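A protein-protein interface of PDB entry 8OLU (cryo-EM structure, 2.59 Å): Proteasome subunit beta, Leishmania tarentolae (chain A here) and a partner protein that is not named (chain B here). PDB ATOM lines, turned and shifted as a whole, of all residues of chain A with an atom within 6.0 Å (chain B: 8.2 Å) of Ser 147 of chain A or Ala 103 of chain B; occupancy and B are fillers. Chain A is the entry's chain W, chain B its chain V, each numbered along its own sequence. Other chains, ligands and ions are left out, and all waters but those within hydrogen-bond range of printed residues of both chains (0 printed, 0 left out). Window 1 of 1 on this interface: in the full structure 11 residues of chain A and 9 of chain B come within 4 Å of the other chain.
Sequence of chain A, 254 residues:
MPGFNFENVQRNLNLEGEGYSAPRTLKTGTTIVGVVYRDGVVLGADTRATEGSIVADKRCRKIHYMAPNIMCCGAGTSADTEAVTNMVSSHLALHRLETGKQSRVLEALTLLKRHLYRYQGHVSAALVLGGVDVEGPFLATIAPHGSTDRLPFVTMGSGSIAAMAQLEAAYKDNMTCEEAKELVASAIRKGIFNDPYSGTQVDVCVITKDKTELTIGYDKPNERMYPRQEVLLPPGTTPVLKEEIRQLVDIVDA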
ATOM      1  N   LYS A 113      19.873 -22.485 -23.847  1.00  0.00           N
ATOM      2  CA  LYS A 113      20.466 -21.166 -23.947  1.00  0.00           C
ATOM      3  C   LYS A 113      20.825 -20.799 -25.376  1.00  0.00           C
ATOM      4  O   LYS A 113      20.801 -19.649 -25.747  1.00  0.00           O
ATOM      5  CB  LYS A 113      21.634 -21.012 -22.984  1.00  0.00           C
ATOM      6  CG  LYS A 113      22.931 -21.578 -23.464  1.00  0.00           C
ATOM      7  CD  LYS A 113      24.005 -21.530 -22.414  1.00  0.00           C
ATOM      8  CE  LYS A 113      24.288 -20.110 -21.976  1.00  0.00           C
ATOM      9  NZ  LYS A 113      25.198 -20.114 -20.797  1.00  0.00           N
ATOM     10  N   THR A 141      19.242 -21.787 -13.899  1.00  0.00           N
ATOM     11  CA  THR A 141      18.283 -20.936 -14.536  1.00  0.00           C
ATOM     12  C   THR A 141      18.670 -20.615 -15.935  1.00  0.00           C
ATOM     13  O   THR A 141      19.831 -20.512 -16.187  1.00  0.00           O
ATOM     14  CB  THR A 141      18.085 -19.617 -13.819  1.00  0.00           C
ATOM     15  OG1 THR A 141      19.243 -19.003 -13.239  1.00  0.00           O
ATOM     16  CG2 THR A 141      17.143 -19.856 -12.650  1.00  0.00           C
ATOM     17  N   ILE A 142      17.717 -20.559 -16.846  1.00  0.00           N
ATOM     18  CA  ILE A 142      17.970 -19.873 -18.083  1.00  0.00           C
ATOM     19  C   ILE A 142      17.076 -18.666 -18.155  1.00  0.00           C
ATOM     20  O   ILE A 142      15.892 -18.742 -17.991  1.00  0.00           O
ATOM     21  CB  ILE A 142      17.808 -20.758 -19.321  1.00  0.00           C
ATOM     22  CG1 ILE A 142      18.628 -22.039 -19.220  1.00  0.00           C
ATOM     23  CG2 ILE A 142      18.308 -20.019 -20.559  1.00  0.00           C
ATOM     24  CD1 ILE A 142      18.017 -23.030 -18.345  1.00  0.00           C
ATOM     25  N   ALA A 143      17.674 -17.534 -18.418  1.00  0.00           N
ATOM     26  CA  ALA A 143      16.916 -16.316 -18.588  1.00  0.00           C
ATOM     27  C   ALA A 143      16.548 -16.179 -20.044  1.00  0.00           C
ATOM     28  O   ALA A 143      17.126 -16.767 -20.911  1.00  0.00           O
ATOM     29  CB  ALA A 143      17.680 -15.134 -18.128  1.00  0.00           C
ATOM     30  N   PRO A 144      15.538 -15.377 -20.367  1.00  0.00           N
ATOM     31  CA  PRO A 144      15.114 -15.255 -21.754  1.00  0.00           C
ATOM     32  C   PRO A 144      16.218 -14.840 -22.690  1.00  0.00           C
ATOM     33  O   PRO A 144      16.212 -15.292 -23.819  1.00  0.00           O
ATOM     34  CB  PRO A 144      14.140 -14.103 -21.696  1.00  0.00           C
ATOM     35  CG  PRO A 144      13.585 -14.200 -20.287  1.00  0.00           C
ATOM     36  CD  PRO A 144      14.786 -14.524 -19.431  1.00  0.00           C
ATOM     37  N   HIS A 145      17.156 -13.989 -22.269  1.00  0.00           N
ATOM     38  CA  HIS A 145      18.185 -13.612 -23.226  1.00  0.00           C
ATOM     39  C   HIS A 145      19.195 -14.725 -23.389  1.00  0.00           C
ATOM     40  O   HIS A 145      20.020 -14.648 -24.278  1.00  0.00           O
ATOM     41  CB  HIS A 145      18.851 -12.288 -22.868  1.00  0.00           C
ATOM     42  CG  HIS A 145      17.922 -11.148 -23.036  1.00  0.00           C
ATOM     43  ND1 HIS A 145      16.957 -10.829 -22.089  1.00  0.00           N
ATOM     44  CD2 HIS A 145      17.759 -10.337 -24.136  1.00  0.00           C
ATOM     45  CE1 HIS A 145      16.222  -9.817 -22.570  1.00  0.00           C
ATOM     46  NE2 HIS A 145      16.712  -9.493 -23.851  1.00  0.00           N
ATOM     47  N   GLY A 146      19.133 -15.741 -22.558  1.00  0.00           N
ATOM     48  CA  GLY A 146      19.929 -16.926 -22.797  1.00  0.00           C
ATOM     49  C   GLY A 146      21.136 -16.960 -21.887  1.00  0.00           C
ATOM     50  O   GLY A 146      22.146 -17.560 -22.220  1.00  0.00           O
ATOM     51  N   SER A 147      21.100 -16.214 -20.800  1.00  0.00           N
ATOM     52  CA  SER A 147      22.102 -16.387 -19.770  1.00  0.00           C
ATOM     53  C   SER A 147      21.691 -17.566 -18.914  1.00  0.00           C
ATOM     54  O   SER A 147      20.539 -17.653 -18.557  1.00  0.00           O
ATOM     55  CB  SER A 147      22.237 -15.171 -18.912  1.00  0.00           C
ATOM     56  OG  SER A 147      20.941 -14.614 -18.599  1.00  0.00           O
ATOM     57  N   THR A 148      22.660 -18.347 -18.484  1.00  0.00           N
ATOM     58  CA  THR A 148      22.454 -19.313 -17.442  1.00  0.00           C
ATOM     59  C   THR A 148      23.237 -19.000 -16.196  1.00  0.00           C
ATOM     60  O   THR A 148      24.267 -18.336 -16.235  1.00  0.00           O
ATOM     61  CB  THR A 148      23.012 -20.682 -17.816  1.00  0.00           C
ATOM     62  OG1 THR A 148      24.437 -20.773 -17.608  1.00  0.00           O
ATOM     63  CG2 THR A 148      22.666 -21.031 -19.257  1.00  0.00           C
ATOM     64  N   ASP A 149      22.784 -19.620 -15.124  1.00  0.00           N
ATOM     65  CA  ASP A 149      23.360 -19.475 -13.809  1.00  0.00           C
ATOM     66  C   ASP A 149      23.110 -20.785 -13.086  1.00  0.00           C
ATOM     67  O   ASP A 149      22.062 -20.992 -12.550  1.00  0.00           O
ATOM     68  CB  ASP A 149      22.709 -18.354 -12.986  1.00  0.00           C
ATOM     69  CG  ASP A 149      23.008 -16.862 -13.327  1.00  0.00           C
ATOM     70  OD1 ASP A 149      24.248 -16.479 -13.564  1.00  0.00           O
ATOM     71  OD2 ASP A 149      22.010 -16.001 -13.243  1.00  0.00           O
ATOM     72  N   THR B  55      29.311  -5.078 -11.597  1.00  0.00           N
ATOM     73  CA  THR B  55      30.411  -5.987 -11.986  1.00  0.00           C
ATOM     74  C   THR B  55      31.703  -5.234 -11.773  1.00  0.00           C
ATOM     75  O   THR B  55      31.796  -4.080 -12.117  1.00  0.00           O
ATOM     76  CB  THR B  55      30.132  -6.411 -13.433  1.00  0.00           C
ATOM     77  OG1 THR B  55      28.942  -7.230 -13.420  1.00  0.00           O
ATOM     78  CG2 THR B  55      31.340  -7.101 -14.054  1.00  0.00           C
ATOM     79  N   THR B  74      25.386 -10.611 -10.085  1.00  0.00           N
ATOM     80  CA  THR B  74      24.698 -10.285 -11.297  1.00  0.00           C
ATOM     81  C   THR B  74      23.429  -9.604 -10.895  1.00  0.00           C
ATOM     82  O   THR B  74      22.674 -10.198 -10.190  1.00  0.00           O
ATOM     83  CB  THR B  74      24.452 -11.576 -12.094  1.00  0.00           C
ATOM     84  OG1 THR B  74      25.698 -12.068 -12.631  1.00  0.00           O
ATOM     85  CG2 THR B  74      23.500 -11.479 -13.276  1.00  0.00           C
ATOM     86  N   SER B  75      23.175  -8.403 -11.377  1.00  0.00           N
ATOM     87  CA  SER B  75      22.019  -7.662 -10.923  1.00  0.00           C
ATOM     88  C   SER B  75      21.133  -7.310 -12.090  1.00  0.00           C
ATOM     89  O   SER B  75      21.620  -6.892 -13.129  1.00  0.00           O
ATOM     90  CB  SER B  75      22.374  -6.414 -10.134  1.00  0.00           C
ATOM     91  OG  SER B  75      23.303  -5.584 -10.799  1.00  0.00           O
ATOM     92  N   VAL B  81      20.102 -11.077  -8.891  1.00  0.00           N
ATOM     93  CA  VAL B  81      19.630 -12.375  -9.305  1.00  0.00           C
ATOM     94  C   VAL B  81      20.657 -13.437  -8.987  1.00  0.00           C
ATOM     95  O   VAL B  81      20.356 -14.567  -8.643  1.00  0.00           O
ATOM     96  CB  VAL B  81      19.219 -12.439 -10.785  1.00  0.00           C
ATOM     97  CG1 VAL B  81      17.833 -11.864 -10.924  1.00  0.00           C
ATOM     98  CG2 VAL B  81      20.131 -11.692 -11.732  1.00  0.00           C
ATOM     99  N   SER B  85      27.874 -15.434  -9.150  1.00  0.00           N
ATOM    100  CA  SER B  85      28.217 -15.681 -10.519  1.00  0.00           C
ATOM    101  C   SER B  85      29.708 -15.846 -10.634  1.00  0.00           C
ATOM    102  O   SER B  85      30.457 -15.541  -9.713  1.00  0.00           O
ATOM    103  CB  SER B  85      27.669 -14.633 -11.418  1.00  0.00           C
ATOM    104  OG  SER B  85      28.282 -13.409 -11.221  1.00  0.00           O
ATOM    105  N   LYS B  87      32.511 -14.911 -13.178  1.00  0.00           N
ATOM    106  CA  LYS B  87      32.696 -14.062 -14.322  1.00  0.00           C
ATOM    107  C   LYS B  87      34.066 -14.299 -14.887  1.00  0.00           C
ATOM    108  O   LYS B  87      34.353 -13.742 -15.900  1.00  0.00           O
ATOM    109  CB  LYS B  87      32.510 -12.614 -13.906  1.00  0.00           C
ATOM    110  CG  LYS B  87      31.120 -12.241 -13.417  1.00  0.00           C
ATOM    111  CD  LYS B  87      31.146 -10.869 -12.749  1.00  0.00           C
ATOM    112  CE  LYS B  87      29.759 -10.455 -12.240  1.00  0.00           C
ATOM    113  NZ  LYS B  87      29.866  -9.185 -11.452  1.00  0.00           N
ATOM    114  N   ARG B  99      34.219 -11.299 -17.734  1.00  0.00           N
ATOM    115  CA  ARG B  99      33.109 -10.855 -18.511  1.00  0.00           C
ATOM    116  C   ARG B  99      32.453  -9.736 -17.740  1.00  0.00           C
ATOM    117  O   ARG B  99      32.264  -9.859 -16.538  1.00  0.00           O
ATOM    118  CB  ARG B  99      32.158 -12.048 -18.652  1.00  0.00           C
ATOM    119  CG  ARG B  99      32.728 -13.274 -19.360  1.00  0.00           C
ATOM    120  CD  ARG B  99      31.718 -14.395 -19.486  1.00  0.00           C
ATOM    121  NE  ARG B  99      31.392 -15.088 -18.250  1.00  0.00           N
ATOM    122  CZ  ARG B  99      30.269 -14.858 -17.593  1.00  0.00           C
ATOM    123  NH1 ARG B  99      29.948 -15.483 -16.476  1.00  0.00           N
ATOM    124  NH2 ARG B  99      29.459 -13.966 -18.125  1.00  0.00           N
ATOM    125  N   SER B 100      32.055  -8.701 -18.452  1.00  0.00           N
ATOM    126  CA  SER B 100      31.130  -7.713 -17.923  1.00  0.00           C
ATOM    127  C   SER B 100      30.152  -7.284 -18.996  1.00  0.00           C
ATOM    128  O   SER B 100      30.457  -7.301 -20.174  1.00  0.00           O
ATOM    129  CB  SER B 100      31.859  -6.492 -17.481  1.00  0.00           C
ATOM    130  OG  SER B 100      32.661  -5.974 -18.572  1.00  0.00           O
ATOM    131  N   GLY B 101      29.038  -6.722 -18.550  1.00  0.00           N
ATOM    132  CA  GLY B 101      27.928  -6.433 -19.434  1.00  0.00           C
ATOM    133  C   GLY B 101      26.924  -7.564 -19.367  1.00  0.00           C
ATOM    134  O   GLY B 101      26.777  -8.253 -18.352  1.00  0.00           O
ATOM    135  N   SER B 102      26.326  -7.807 -20.509  1.00  0.00           N
ATOM    136  CA  SER B 102      25.173  -8.657 -20.572  1.00  0.00           C
ATOM    137  C   SER B 102      25.682 -10.062 -20.400  1.00  0.00           C
ATOM    138  O   SER B 102      26.503 -10.514 -21.162  1.00  0.00           O
ATOM    139  CB  SER B 102      24.485  -8.441 -21.873  1.00  0.00           C
ATOM    140  OG  SER B 102      23.558  -9.481 -22.213  1.00  0.00           O
ATOM    141  N   ALA B 103      25.202 -10.720 -19.364  1.00  0.00           N
ATOM    142  CA  ALA B 103      25.590 -12.083 -19.079  1.00  0.00           C
ATOM    143  C   ALA B 103      25.324 -12.887 -20.333  1.00  0.00           C
ATOM    144  O   ALA B 103      26.120 -13.710 -20.761  1.00  0.00           O
ATOM    145  CB  ALA B 103      24.781 -12.552 -17.902  1.00  0.00           C
ATOM    146  N   ALA B 104      24.181 -12.639 -20.937  1.00  0.00           N
ATOM    147  CA  ALA B 104      23.827 -13.470 -22.055  1.00  0.00           C
ATOM    148  C   ALA B 104      24.882 -13.346 -23.140  1.00  0.00           C
ATOM    149  O   ALA B 104      25.309 -14.337 -23.716  1.00  0.00           O
ATOM    150  CB  ALA B 104      22.475 -13.072 -22.600  1.00  0.00           C
ATOM    151  N   ASP B 105      25.173 -12.096 -23.461  1.00  0.00           N
ATOM    152  CA  ASP B 105      26.067 -11.792 -24.544  1.00  0.00           C
ATOM    153  C   ASP B 105      27.440 -12.347 -24.253  1.00  0.00           C
ATOM    154  O   ASP B 105      28.060 -12.883 -25.138  1.00  0.00           O
ATOM    155  CB  ASP B 105      26.163 -10.278 -24.762  1.00  0.00           C
ATOM    156  CG  ASP B 105      24.886  -9.691 -25.352  1.00  0.00           C
ATOM    157  OD1 ASP B 105      24.364 -10.323 -26.365  1.00  0.00           O
ATOM    158  OD2 ASP B 105      24.426  -8.593 -24.853  1.00  0.00           O
ATOM    159  N   THR B 106      27.916 -12.141 -23.062  1.00  0.00           N
ATOM    160  CA  THR B 106      29.270 -12.506 -22.768  1.00  0.00           C
ATOM    161  C   THR B 106      29.446 -14.004 -22.632  1.00  0.00           C
ATOM    162  O   THR B 106      30.487 -14.525 -22.981  1.00  0.00           O
ATOM    163  CB  THR B 106      29.741 -11.887 -21.453  1.00  0.00           C
ATOM    164  OG1 THR B 106      28.956 -12.224 -20.302  1.00  0.00           O
ATOM    165  CG2 THR B 106      29.814 -10.383 -21.597  1.00  0.00           C
ATOM    166  N   GLN B 107      28.428 -14.675 -22.109  1.00  0.00           N
ATOM    167  CA  GLN B 107      28.473 -16.109 -22.073  1.00  0.00           C
ATOM    168  C   GLN B 107      28.426 -16.635 -23.497  1.00  0.00           C
ATOM    169  O   GLN B 107      29.115 -17.600 -23.805  1.00  0.00           O
ATOM    170  CB  GLN B 107      27.329 -16.687 -21.263  1.00  0.00           C
ATOM    171  CG  GLN B 107      27.411 -16.403 -19.769  1.00  0.00           C
ATOM    172  CD  GLN B 107      26.183 -16.943 -19.063  1.00  0.00           C
ATOM    173  OE1 GLN B 107      25.478 -17.752 -19.633  1.00  0.00           O
ATOM    174  NE2 GLN B 107      25.886 -16.501 -17.846  1.00  0.00           N
ATOM    175  N   ALA B 108      27.629 -16.044 -24.372  1.00  0.00           N
ATOM    176  CA  ALA B 108      27.575 -16.581 -25.701  1.00  0.00           C
ATOM    177  C   ALA B 108      28.902 -16.390 -26.375  1.00  0.00           C
ATOM    178  O   ALA B 108      29.297 -17.278 -27.110  1.00  0.00           O
ATOM    179  CB  ALA B 108      26.528 -15.938 -26.524  1.00  0.00           C
ATOM    180  N   LEU B 109      29.576 -15.255 -26.199  1.00  0.00           N
ATOM    181  CA  LEU B 109      30.833 -15.074 -26.887  1.00  0.00           C
ATOM    182  C   LEU B 109      31.921 -15.938 -26.301  1.00  0.00           C
ATOM    183  O   LEU B 109      32.875 -16.251 -26.929  1.00  0.00           O
ATOM    184  CB  LEU B 109      31.293 -13.643 -26.726  1.00  0.00           C
ATOM    185  CG  LEU B 109      30.487 -12.606 -27.487  1.00  0.00           C
ATOM    186  CD1 LEU B 109      30.902 -11.202 -27.056  1.00  0.00           C
ATOM    187  CD2 LEU B 109      30.650 -12.787 -28.979  1.00  0.00           C
ATOM    188  N   ALA B 110      31.925 -16.093 -25.019  1.00  0.00           N
ATOM    189  CA  ALA B 110      32.993 -16.831 -24.419  1.00  0.00           C
ATOM    190  C   ALA B 110      32.864 -18.270 -24.890  1.00  0.00           C
ATOM    191  O   ALA B 110      33.865 -18.935 -25.066  1.00  0.00           O
ATOM    192  CB  ALA B 110      32.902 -16.683 -22.912  1.00  0.00           C
ATOM    193  N   GLU B 111      31.633 -18.768 -25.046  1.00  0.00           N
ATOM    194  CA  GLU B 111      31.451 -20.173 -25.354  1.00  0.00           C
ATOM    195  C   GLU B 111      31.883 -20.361 -26.794  1.00  0.00           C
ATOM    196  O   GLU B 111      32.535 -21.323 -27.133  1.00  0.00           O
ATOM    197  CB  GLU B 111      30.006 -20.605 -25.158  1.00  0.00           C
ATOM    198  CG  GLU B 111      29.698 -21.075 -23.740  1.00  0.00           C
ATOM    199  CD  GLU B 111      28.280 -20.895 -23.126  1.00  0.00           C
ATOM    200  OE1 GLU B 111      27.336 -20.261 -23.781  1.00  0.00           O
ATOM    201  OE2 GLU B 111      28.098 -21.379 -21.933  1.00  0.00           O
ATOM    202  N   SER B 149      26.227  -5.781 -25.245  1.00  0.00           N
ATOM    203  CA  SER B 149      26.891  -5.005 -24.230  1.00  0.00           C
ATOM    204  C   SER B 149      27.935  -5.928 -23.639  1.00  0.00           C
ATOM    205  O   SER B 149      27.588  -7.002 -23.148  1.00  0.00           O
ATOM    206  CB  SER B 149      25.904  -4.506 -23.173  1.00  0.00           C
ATOM    207  OG  SER B 149      26.290  -4.846 -21.819  1.00  0.00           O
ATOM    208  N   ALA B 150      29.212  -5.575 -23.749  1.00  0.00           N
ATOM    209  CA  ALA B 150      30.217  -6.583 -23.462  1.00  0.00           C
ATOM    210  C   ALA B 150      31.547  -5.902 -23.253  1.00  0.00           C
ATOM    211  O   ALA B 150      32.153  -5.397 -24.208  1.00  0.00           O
ATOM    212  CB  ALA B 150      30.283  -7.580 -24.587  1.00  0.00           C
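Among the printed residues, merely in contact across the chains: His 145 of chain A with Ala 104 of chain B, Ser 147 of chain A with Gln 107 of chain B, Ser 147 of chain A with Ala 104 of chain B and Ser 147 of chain A with Ala 103 of chain B.
Of the 10 printed residues of chain A, 4 touch a printed residue of chain B.
Printed residues of chain A that touch a printed residue of chain B: Lys 113, His 145, Ser 147 and Thr 148.
Among the printed residues, Asp or Glu carboxylates within 4 Å of a Lys or Arg side-chain nitrogen of the other chain: Lys 113 of chain A with Glu 111 of chain B (3.4 Å).
The side-chain amino group (NZ) of Lys 113 of chain A lies within salt-bridge range of the side-chain carboxylate (OE2) of Glu 111 of chain B (3.4 Å).
The side-chain amide oxygen of Gln 107 of chain B lies within hydrogen-bond range of the side-chain amino group of Lys 113 of chain A (2.6 Å).
NE2 of Gln 107 of chain B lies within hydrogen-bond range of O of Thr 148 of chain A (2.9 Å).
NZ of Lys 113 of chain A lies close to OG1 of Thr 148 of chain A, at 3.3 Å.
The side-chain hydroxyl of Ser 102 of chain B lies close to the backbone NH of Ala 104 of chain B (3.5 Å).
The side-chain hydroxyl of Thr 106 of chain B is in hydrogen-bond range of the backbone carbonyl oxygen of Ala 103 of chain B.
Printed residues of chain B within 4 Å of Lys 113 of chain A: Gln 107 and Glu 111.
Of the printed residues of chain B, His 145 of chain A touches Ala 104.
No residue of chain B comes within 4 Å of Gly 146 of chain A.
Of chain B, only Ala 103 (3.8 Å), Ala 104 (3.8 Å) and Gln 107 (3.6 Å) come within 4 Å of Ser 147 of chain A.
Ala 103 of chain B touches one residue of chain A.
Printed residues of chain A within 4 Å of Ala 104 of chain B: His 145 and Ser 147.
Printed residues of chain A within 4 Å of Gln 107 of chain B: Lys 113 (2.6 Å), Ser 147 (3.6 Å) and Thr 148 (2.9 Å).
Printed residues of chain A within 4 Å of Glu 111 of chain B: Lys 113 (3.4 Å).
The nearest residue of chain B that does not touch Ser 147 of chain A is Asp 105 of chain B (6.2 Å).
The nearest printed residue of chain B that does not touch Lys 113 of chain A is Ala 108 of chain B (5.8 Å).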
